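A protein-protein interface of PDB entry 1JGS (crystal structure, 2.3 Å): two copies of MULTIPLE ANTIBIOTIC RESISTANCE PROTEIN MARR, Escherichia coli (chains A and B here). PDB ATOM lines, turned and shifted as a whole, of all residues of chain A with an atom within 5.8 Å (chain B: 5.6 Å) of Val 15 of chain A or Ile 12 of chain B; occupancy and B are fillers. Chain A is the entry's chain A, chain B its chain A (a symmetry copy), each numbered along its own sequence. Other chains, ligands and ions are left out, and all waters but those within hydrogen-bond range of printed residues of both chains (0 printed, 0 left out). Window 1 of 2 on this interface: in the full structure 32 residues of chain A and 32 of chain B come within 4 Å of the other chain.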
ATOM      1  N   ARG A  10     -23.598   4.234   7.120  1.00  0.00           N
ATOM      2  CA  ARG A  10     -23.896   2.830   7.378  1.00  0.00           C
ATOM      3  C   ARG A  10     -23.143   2.321   8.605  1.00  0.00           C
ATOM      4  O   ARG A  10     -23.680   1.526   9.376  1.00  0.00           O
ATOM      5  CB  ARG A  10     -23.546   1.975   6.158  1.00  0.00           C
ATOM      6  CG  ARG A  10     -24.578   2.019   5.038  1.00  0.00           C
ATOM      7  CD  ARG A  10     -24.035   1.345   3.783  1.00  0.00           C
ATOM      8  NE  ARG A  10     -23.597  -0.030   4.031  1.00  0.00           N
ATOM      9  CZ  ARG A  10     -22.806  -0.722   3.214  1.00  0.00           C
ATOM     10  NH1 ARG A  10     -22.359  -0.172   2.092  1.00  0.00           N
ATOM     11  NH2 ARG A  10     -22.459  -1.966   3.518  1.00  0.00           N
ATOM     12  N   LEU A  11     -21.902   2.773   8.793  1.00  0.00           N
ATOM     13  CA  LEU A  11     -21.130   2.334   9.949  1.00  0.00           C
ATOM     14  C   LEU A  11     -21.806   2.796  11.240  1.00  0.00           C
ATOM     15  O   LEU A  11     -21.905   2.031  12.193  1.00  0.00           O
ATOM     16  CB  LEU A  11     -19.690   2.862   9.891  1.00  0.00           C
ATOM     17  CG  LEU A  11     -18.745   2.213   8.872  1.00  0.00           C
ATOM     18  CD1 LEU A  11     -17.365   2.875   8.927  1.00  0.00           C
ATOM     19  CD2 LEU A  11     -18.632   0.735   9.171  1.00  0.00           C
ATOM     20  N   ILE A  12     -22.244   4.052  11.271  1.00  0.00           N
ATOM     21  CA  ILE A  12     -22.933   4.595  12.441  1.00  0.00           C
ATOM     22  C   ILE A  12     -24.182   3.739  12.677  1.00  0.00           C
ATOM     23  O   ILE A  12     -24.540   3.440  13.819  1.00  0.00           O
ATOM     24  CB  ILE A  12     -23.382   6.059  12.213  1.00  0.00           C
ATOM     25  CG1 ILE A  12     -22.162   6.977  12.134  1.00  0.00           C
ATOM     26  CG2 ILE A  12     -24.273   6.517  13.350  1.00  0.00           C
ATOM     27  CD1 ILE A  12     -22.518   8.427  11.807  1.00  0.00           C
ATOM     28  N   HIS A  13     -24.830   3.346  11.584  1.00  0.00           N
ATOM     29  CA  HIS A  13     -26.029   2.527  11.648  1.00  0.00           C
ATOM     30  C   HIS A  13     -25.679   1.205  12.304  1.00  0.00           C
ATOM     31  O   HIS A  13     -26.137   0.900  13.408  1.00  0.00           O
ATOM     32  CB  HIS A  13     -26.560   2.289  10.236  1.00  0.00           C
ATOM     33  CG  HIS A  13     -27.739   1.370  10.171  1.00  0.00           C
ATOM     34  ND1 HIS A  13     -28.903   1.597  10.873  1.00  0.00           N
ATOM     35  CD2 HIS A  13     -27.950   0.243   9.451  1.00  0.00           C
ATOM     36  CE1 HIS A  13     -29.780   0.652  10.588  1.00  0.00           C
ATOM     37  NE2 HIS A  13     -29.227  -0.183   9.726  1.00  0.00           N
ATOM     38  N   MET A  14     -24.853   0.429  11.613  1.00  0.00           N
ATOM     39  CA  MET A  14     -24.406  -0.872  12.100  1.00  0.00           C
ATOM     40  C   MET A  14     -23.991  -0.840  13.564  1.00  0.00           C
ATOM     41  O   MET A  14     -24.266  -1.780  14.296  1.00  0.00           O
ATOM     42  CB  MET A  14     -23.216  -1.365  11.273  1.00  0.00           C
ATOM     43  CG  MET A  14     -23.539  -1.770   9.849  1.00  0.00           C
ATOM     44  SD  MET A  14     -22.021  -2.120   8.917  1.00  0.00           S
ATOM     45  CE  MET A  14     -21.560  -3.741   9.593  1.00  0.00           C
ATOM     46  N   VAL A  15     -23.311   0.225  13.985  1.00  0.00           N
ATOM     47  CA  VAL A  15     -22.857   0.343  15.370  1.00  0.00           C
ATOM     48  C   VAL A  15     -23.999   0.623  16.348  1.00  0.00           C
ATOM     49  O   VAL A  15     -23.994   0.130  17.491  1.00  0.00           O
ATOM     50  CB  VAL A  15     -21.801   1.457  15.535  1.00  0.00           C
ATOM     51  CG1 VAL A  15     -21.388   1.551  16.997  1.00  0.00           C
ATOM     52  CG2 VAL A  15     -20.569   1.155  14.656  1.00  0.00           C
ATOM     53  N   ASN A  16     -24.965   1.428  15.913  1.00  0.00           N
ATOM     54  CA  ASN A  16     -26.096   1.736  16.772  1.00  0.00           C
ATOM     55  C   ASN A  16     -26.849   0.428  16.897  1.00  0.00           C
ATOM     56  O   ASN A  16     -27.320   0.063  17.978  1.00  0.00           O
ATOM     57  CB  ASN A  16     -27.006   2.796  16.151  1.00  0.00           C
ATOM     58  CG  ASN A  16     -28.009   3.343  17.150  1.00  0.00           C
ATOM     59  OD1 ASN A  16     -27.629   3.952  18.149  1.00  0.00           O
ATOM     60  ND2 ASN A  16     -29.296   3.121  16.889  1.00  0.00           N
ATOM     61  N   GLN A  17     -26.941  -0.277  15.773  1.00  0.00           N
ATOM     62  CA  GLN A  17     -27.615  -1.565  15.721  1.00  0.00           C
ATOM     63  C   GLN A  17     -27.022  -2.400  16.848  1.00  0.00           C
ATOM     64  O   GLN A  17     -27.709  -2.747  17.808  1.00  0.00           O
ATOM     65  CB  GLN A  17     -27.348  -2.234  14.372  1.00  0.00           C
ATOM     66  CG  GLN A  17     -28.242  -3.420  14.049  1.00  0.00           C
ATOM     67  CD  GLN A  17     -29.182  -3.139  12.884  1.00  0.00           C
ATOM     68  OE1 GLN A  17     -28.742  -2.862  11.762  1.00  0.00           O
ATOM     69  NE2 GLN A  17     -30.486  -3.210  13.145  1.00  0.00           N
ATOM     70  N   LYS A  18     -25.729  -2.687  16.734  1.00  0.00           N
ATOM     71  CA  LYS A  18     -25.014  -3.479  17.726  1.00  0.00           C
ATOM     72  C   LYS A  18     -25.343  -3.014  19.136  1.00  0.00           C
ATOM     73  O   LYS A  18     -25.695  -3.815  19.997  1.00  0.00           O
ATOM     74  CB  LYS A  18     -23.500  -3.382  17.512  1.00  0.00           C
ATOM     75  CG  LYS A  18     -22.713  -4.273  18.461  1.00  0.00           C
ATOM     76  CD  LYS A  18     -21.243  -3.909  18.517  1.00  0.00           C
ATOM     77  CE  LYS A  18     -20.466  -4.830  19.467  1.00  0.00           C
ATOM     78  NZ  LYS A  18     -19.841  -6.000  18.773  1.00  0.00           N
ATOM     79  N   LYS A  19     -25.216  -1.713  19.356  1.00  0.00           N
ATOM     80  CA  LYS A  19     -25.477  -1.106  20.658  1.00  0.00           C
ATOM     81  C   LYS A  19     -26.843  -1.495  21.221  1.00  0.00           C
ATOM     82  O   LYS A  19     -26.979  -1.764  22.417  1.00  0.00           O
ATOM     83  CB  LYS A  19     -25.363   0.419  20.541  1.00  0.00           C
ATOM     84  CG  LYS A  19     -25.459   1.179  21.855  1.00  0.00           C
ATOM     85  CD  LYS A  19     -26.859   1.722  22.092  1.00  0.00           C
ATOM     86  CE  LYS A  19     -26.890   2.625  23.320  1.00  0.00           C
ATOM     87  NZ  LYS A  19     -28.207   3.296  23.509  1.00  0.00           N
ATOM     88  N   ASP A  20     -27.855  -1.532  20.362  1.00  0.00           N
ATOM     89  CA  ASP A  20     -29.184  -1.883  20.831  1.00  0.00           C
ATOM     90  C   ASP A  20     -29.261  -3.367  21.125  1.00  0.00           C
ATOM     91  O   ASP A  20     -29.881  -3.777  22.111  1.00  0.00           O
ATOM     92  CB  ASP A  20     -30.252  -1.481  19.808  1.00  0.00           C
ATOM     93  CG  ASP A  20     -30.489   0.026  19.771  1.00  0.00           C
ATOM     94  OD1 ASP A  20     -30.376   0.682  20.834  1.00  0.00           O
ATOM     95  OD2 ASP A  20     -30.803   0.552  18.681  1.00  0.00           O
ATOM     96  N   LEU A 117     -18.469  -2.331  24.144  1.00  0.00           N
ATOM     97  CA  LEU A 117     -18.190  -1.482  22.987  1.00  0.00           C
ATOM     98  C   LEU A 117     -16.710  -1.145  22.889  1.00  0.00           C
ATOM     99  O   LEU A 117     -16.134  -1.093  21.799  1.00  0.00           O
ATOM    100  CB  LEU A 117     -18.978  -0.169  23.079  1.00  0.00           C
ATOM    101  CG  LEU A 117     -20.502  -0.215  23.004  1.00  0.00           C
ATOM    102  CD1 LEU A 117     -21.068   1.190  23.167  1.00  0.00           C
ATOM    103  CD2 LEU A 117     -20.912  -0.819  21.668  1.00  0.00           C
ATOM    104  N   LEU A 133     -16.332  11.767  17.105  1.00  0.00           N
ATOM    105  CA  LEU A 133     -17.788  11.689  17.081  1.00  0.00           C
ATOM    106  C   LEU A 133     -18.406  13.009  17.515  1.00  0.00           C
ATOM    107  O   LEU A 133     -19.529  13.331  17.131  1.00  0.00           O
ATOM    108  CB  LEU A 133     -18.289  10.563  17.992  1.00  0.00           C
ATOM    109  CG  LEU A 133     -18.243   9.133  17.438  1.00  0.00           C
ATOM    110  CD1 LEU A 133     -18.700   8.160  18.523  1.00  0.00           C
ATOM    111  CD2 LEU A 133     -19.133   9.017  16.207  1.00  0.00           C
ATOM    112  N   PRO B   7     -19.854   9.681  27.619  1.00  0.00           N
ATOM    113  CA  PRO B   7     -19.527   8.286  27.302  1.00  0.00           C
ATOM    114  C   PRO B   7     -19.932   7.906  25.872  1.00  0.00           C
ATOM    115  O   PRO B   7     -20.958   8.365  25.365  1.00  0.00           O
ATOM    116  CB  PRO B   7     -20.304   7.508  28.363  1.00  0.00           C
ATOM    117  CG  PRO B   7     -21.528   8.368  28.564  1.00  0.00           C
ATOM    118  CD  PRO B   7     -20.923   9.753  28.631  1.00  0.00           C
ATOM    119  N   LEU B   8     -19.122   7.060  25.242  1.00  0.00           N
ATOM    120  CA  LEU B   8     -19.344   6.606  23.869  1.00  0.00           C
ATOM    121  C   LEU B   8     -20.811   6.304  23.541  1.00  0.00           C
ATOM    122  O   LEU B   8     -21.368   6.851  22.574  1.00  0.00           O
ATOM    123  CB  LEU B   8     -18.486   5.365  23.607  1.00  0.00           C
ATOM    124  CG  LEU B   8     -18.527   4.679  22.247  1.00  0.00           C
ATOM    125  CD1 LEU B   8     -18.023   5.614  21.154  1.00  0.00           C
ATOM    126  CD2 LEU B   8     -17.659   3.433  22.317  1.00  0.00           C
ATOM    127  N   GLY B   9     -21.425   5.435  24.347  1.00  0.00           N
ATOM    128  CA  GLY B   9     -22.817   5.069  24.140  1.00  0.00           C
ATOM    129  C   GLY B   9     -23.730   6.240  23.826  1.00  0.00           C
ATOM    130  O   GLY B   9     -24.460   6.215  22.834  1.00  0.00           O
ATOM    131  N   ARG B  10     -23.703   7.267  24.670  1.00  0.00           N
ATOM    132  CA  ARG B  10     -24.545   8.437  24.445  1.00  0.00           C
ATOM    133  C   ARG B  10     -24.125   9.188  23.183  1.00  0.00           C
ATOM    134  O   ARG B  10     -24.975   9.697  22.454  1.00  0.00           O
ATOM    135  CB  ARG B  10     -24.492   9.375  25.653  1.00  0.00           C
ATOM    136  CG  ARG B  10     -25.357   8.941  26.830  1.00  0.00           C
ATOM    137  CD  ARG B  10     -25.054   9.789  28.060  1.00  0.00           C
ATOM    138  NE  ARG B  10     -25.209  11.222  27.803  1.00  0.00           N
ATOM    139  CZ  ARG B  10     -24.710  12.180  28.582  1.00  0.00           C
ATOM    140  NH1 ARG B  10     -24.019  11.864  29.671  1.00  0.00           N
ATOM    141  NH2 ARG B  10     -24.899  13.456  28.273  1.00  0.00           N
ATOM    142  N   LEU B  11     -22.819   9.260  22.920  1.00  0.00           N
ATOM    143  CA  LEU B  11     -22.349   9.954  21.727  1.00  0.00           C
ATOM    144  C   LEU B  11     -22.860   9.248  20.472  1.00  0.00           C
ATOM    145  O   LEU B  11     -23.307   9.901  19.535  1.00  0.00           O
ATOM    146  CB  LEU B  11     -20.817  10.037  21.697  1.00  0.00           C
ATOM    147  CG  LEU B  11     -20.148  11.017  22.670  1.00  0.00           C
ATOM    148  CD1 LEU B  11     -18.625  10.954  22.528  1.00  0.00           C
ATOM    149  CD2 LEU B  11     -20.645  12.417  22.382  1.00  0.00           C
ATOM    150  N   ILE B  12     -22.769   7.921  20.451  1.00  0.00           N
ATOM    151  CA  ILE B  12     -23.252   7.136  19.316  1.00  0.00           C
ATOM    152  C   ILE B  12     -24.749   7.427  19.160  1.00  0.00           C
ATOM    153  O   ILE B  12     -25.260   7.548  18.045  1.00  0.00           O
ATOM    154  CB  ILE B  12     -23.074   5.617  19.551  1.00  0.00           C
ATOM    155  CG1 ILE B  12     -21.588   5.256  19.551  1.00  0.00           C
ATOM    156  CG2 ILE B  12     -23.775   4.832  18.462  1.00  0.00           C
ATOM    157  CD1 ILE B  12     -21.324   3.786  19.881  1.00  0.00           C
ATOM    158  N   HIS B  13     -25.436   7.546  20.293  1.00  0.00           N
ATOM    159  CA  HIS B  13     -26.863   7.825  20.307  1.00  0.00           C
ATOM    160  C   HIS B  13     -27.100   9.170  19.647  1.00  0.00           C
ATOM    161  O   HIS B  13     -27.703   9.256  18.575  1.00  0.00           O
ATOM    162  CB  HIS B  13     -27.364   7.851  21.749  1.00  0.00           C
ATOM    163  CG  HIS B  13     -28.803   8.230  21.892  1.00  0.00           C
ATOM    164  ND1 HIS B  13     -29.821   7.555  21.254  1.00  0.00           N
ATOM    165  CD2 HIS B  13     -29.401   9.192  22.636  1.00  0.00           C
ATOM    166  CE1 HIS B  13     -30.982   8.081  21.600  1.00  0.00           C
ATOM    167  NE2 HIS B  13     -30.756   9.076  22.439  1.00  0.00           N
ATOM    168  N   MET B  14     -26.610  10.217  20.299  1.00  0.00           N
ATOM    169  CA  MET B  14     -26.740  11.583  19.803  1.00  0.00           C
ATOM    170  C   MET B  14     -26.430  11.700  18.318  1.00  0.00           C
ATOM    171  O   MET B  14     -27.095  12.446  17.614  1.00  0.00           O
ATOM    172  CB  MET B  14     -25.797  12.515  20.567  1.00  0.00           C
ATOM    173  CG  MET B  14     -26.171  12.776  22.012  1.00  0.00           C
ATOM    174  SD  MET B  14     -24.864  13.708  22.860  1.00  0.00           S
ATOM    175  CE  MET B  14     -25.119  15.371  22.178  1.00  0.00           C
ATOM    176  N   VAL B  15     -25.410  10.985  17.846  1.00  0.00           N
ATOM    177  CA  VAL B  15     -25.026  11.039  16.437  1.00  0.00           C
ATOM    178  C   VAL B  15     -26.018  10.320  15.522  1.00  0.00           C
ATOM    179  O   VAL B  15     -26.273  10.762  14.386  1.00  0.00           O
ATOM    180  CB  VAL B  15     -23.627  10.430  16.200  1.00  0.00           C
ATOM    181  CG1 VAL B  15     -23.294  10.489  14.715  1.00  0.00           C
ATOM    182  CG2 VAL B  15     -22.566  11.204  17.011  1.00  0.00           C
ATOM    183  N   ASN B  16     -26.562   9.205  16.002  1.00  0.00           N
ATOM    184  CA  ASN B  16     -27.527   8.466  15.205  1.00  0.00           C
ATOM    185  C   ASN B  16     -28.740   9.369  15.138  1.00  0.00           C
ATOM    186  O   ASN B  16     -29.377   9.506  14.089  1.00  0.00           O
ATOM    187  CB  ASN B  16     -27.908   7.140  15.864  1.00  0.00           C
ATOM    188  CG  ASN B  16     -28.669   6.230  14.917  1.00  0.00           C
ATOM    189  OD1 ASN B  16     -28.136   5.808  13.891  1.00  0.00           O
ATOM    190  ND2 ASN B  16     -29.922   5.930  15.253  1.00  0.00           N
ATOM    191  N   GLN B  17     -29.039   9.993  16.273  1.00  0.00           N
ATOM    192  CA  GLN B  17     -30.161  10.912  16.378  1.00  0.00           C
ATOM    193  C   GLN B  17     -30.012  11.900  15.229  1.00  0.00           C
ATOM    194  O   GLN B  17     -30.833  11.937  14.315  1.00  0.00           O
ATOM    195  CB  GLN B  17     -30.105  11.647  17.717  1.00  0.00           C
ATOM    196  CG  GLN B  17     -31.374  12.388  18.105  1.00  0.00           C
ATOM    197  CD  GLN B  17     -32.060  11.773  19.318  1.00  0.00           C
ATOM    198  OE1 GLN B  17     -31.483  11.705  20.410  1.00  0.00           O
ATOM    199  NE2 GLN B  17     -33.298  11.322  19.132  1.00  0.00           N
ATOM    200  N   LEU B 133     -14.634   3.095  14.202  1.00  0.00           N
ATOM    201  CA  LEU B 133     -15.999   2.593  14.309  1.00  0.00           C
ATOM    202  C   LEU B 133     -16.070   1.131  13.896  1.00  0.00           C
ATOM    203  O   LEU B 133     -16.952   0.397  14.339  1.00  0.00           O
ATOM    204  CB  LEU B 133     -16.954   3.419  13.441  1.00  0.00           C
ATOM    205  CG  LEU B 133     -17.445   4.758  14.008  1.00  0.00           C
ATOM    206  CD1 LEU B 133     -18.309   5.459  12.962  1.00  0.00           C
ATOM    207  CD2 LEU B 133     -18.237   4.527  15.289  1.00  0.00           C
ATOM    208  N   VAL B 136     -15.215  -1.457  16.546  1.00  0.00           N
ATOM    209  CA  VAL B 136     -16.269  -1.637  17.536  1.00  0.00           C
ATOM    210  C   VAL B 136     -17.209  -2.790  17.149  1.00  0.00           C
ATOM    211  O   VAL B 136     -17.811  -3.423  18.017  1.00  0.00           O
ATOM    212  CB  VAL B 136     -17.121  -0.347  17.690  1.00  0.00           C
ATOM    213  CG1 VAL B 136     -18.331  -0.624  18.567  1.00  0.00           C
ATOM    214  CG2 VAL B 136     -16.281   0.775  18.288  1.00  0.00           C
ATOM    215  N   LEU B 137     -17.317  -3.071  15.853  1.00  0.00           N
ATOM    216  CA  LEU B 137     -18.219  -4.115  15.363  1.00  0.00           C
ATOM    217  C   LEU B 137     -17.897  -5.595  15.639  1.00  0.00           C
ATOM    218  O   LEU B 137     -18.762  -6.353  16.098  1.00  0.00           O
ATOM    219  CB  LEU B 137     -18.452  -3.915  13.859  1.00  0.00           C
ATOM    220  CG  LEU B 137     -19.270  -2.659  13.563  1.00  0.00           C
ATOM    221  CD1 LEU B 137     -19.523  -2.525  12.087  1.00  0.00           C
ATOM    222  CD2 LEU B 137     -20.576  -2.736  14.325  1.00  0.00           C
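Ile 12 of chain A touches Val 15 of chain B, and with the chains exchanged Val 15 of chain A touches Ile 12 of chain B. Ile 12 of chain A touches Asn 16 of chain B, and with the chains exchanged Asn 16 of chain A touches Ile 12 of chain B. Val 15 of chain A touches Leu 133 of chain B, and with the chains exchanged Leu 133 of chain A touches Val 15 of chain B. Asn 16 of chain A touches its own counterpart, Asn 16 of chain B. 9 positions are printed for both chains. Of the 14 pairs that touch across the chains among the printed residues, 7 have their exchanged pair printed and touching as well.
The side-chain amide nitrogen (ND2) of Asn 16 of chain B lies close to the side-chain amide nitrogen (ND2) of Asn 16 of chain A (3.3 Å). O of Val 136 of chain B lies close to NZ of Lys 18 of chain A, at 3.4 Å. O of Leu 137 of chain B sits at hydrogen-bond distance from NZ of Lys 18 of chain A, at 2.9 Å.
Val 15 of chain A touches just these residues of chain B: Ile 12, Leu 133 and Leu 137. Printed residues of chain A within 4 Å of Ile 12 of chain B: Val 15 and Asn 16. Of the printed residues of chain B, Asn 16 of chain A touches Ile 12 and Asn 16. Of the printed residues of chain B, Leu 117 of chain A touches Leu 8 and Val 136. Lys 19 of chain A touches none of the printed residues of chain B.
Among the printed residues, pairs that only touch across the chains: Met 14 of chain A with Leu 137 of chain B (3.4 Å), Ile 12 of chain A with Val 15 of chain B (3.6 Å), Val 15 of chain A with Ile 12 of chain B (3.6 Å), Val 15 of chain A with Leu 133 of chain B (3.7 Å), Leu 133 of chain A with Val 15 of chain B (3.7 Å), Leu 133 of chain A with Leu 8 of chain B (3.7 Å), Val 15 of chain A with Leu 137 of chain B (3.9 Å), Leu 117 of chain A with Leu 8 of chain B (3.9 Å), Leu 117 of chain A with Val 136 of chain B (3.9 Å), Ile 12 of chain A with Asn 16 of chain B (3.96 Å) and Asn 16 of chain A with Ile 12 of chain B (3.97 Å).
The side-chain amide nitrogen of Asn 16 of chain A lies within hydrogen-bond range of the side-chain carboxylate of Asp 20 of chain A, at 3.5 Å.
Hydrophobic or aromatic side chains of chain B within 4 Å of the printed part of chain A: Leu 8, Ile 12, Val 15, Val 136 and Leu 137. Of the 13 printed residues of chain A, 7 touch a printed residue of chain B. Hydrophobic or aromatic side chains of chain A that line the printed part of chain B: Ile 12, Met 14, Val 15, Leu 117 and Leu 133. Among the printed residues, no Asp or Glu carboxylate lies within 4 Å of a Lys or Arg side-chain nitrogen of the other chain.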
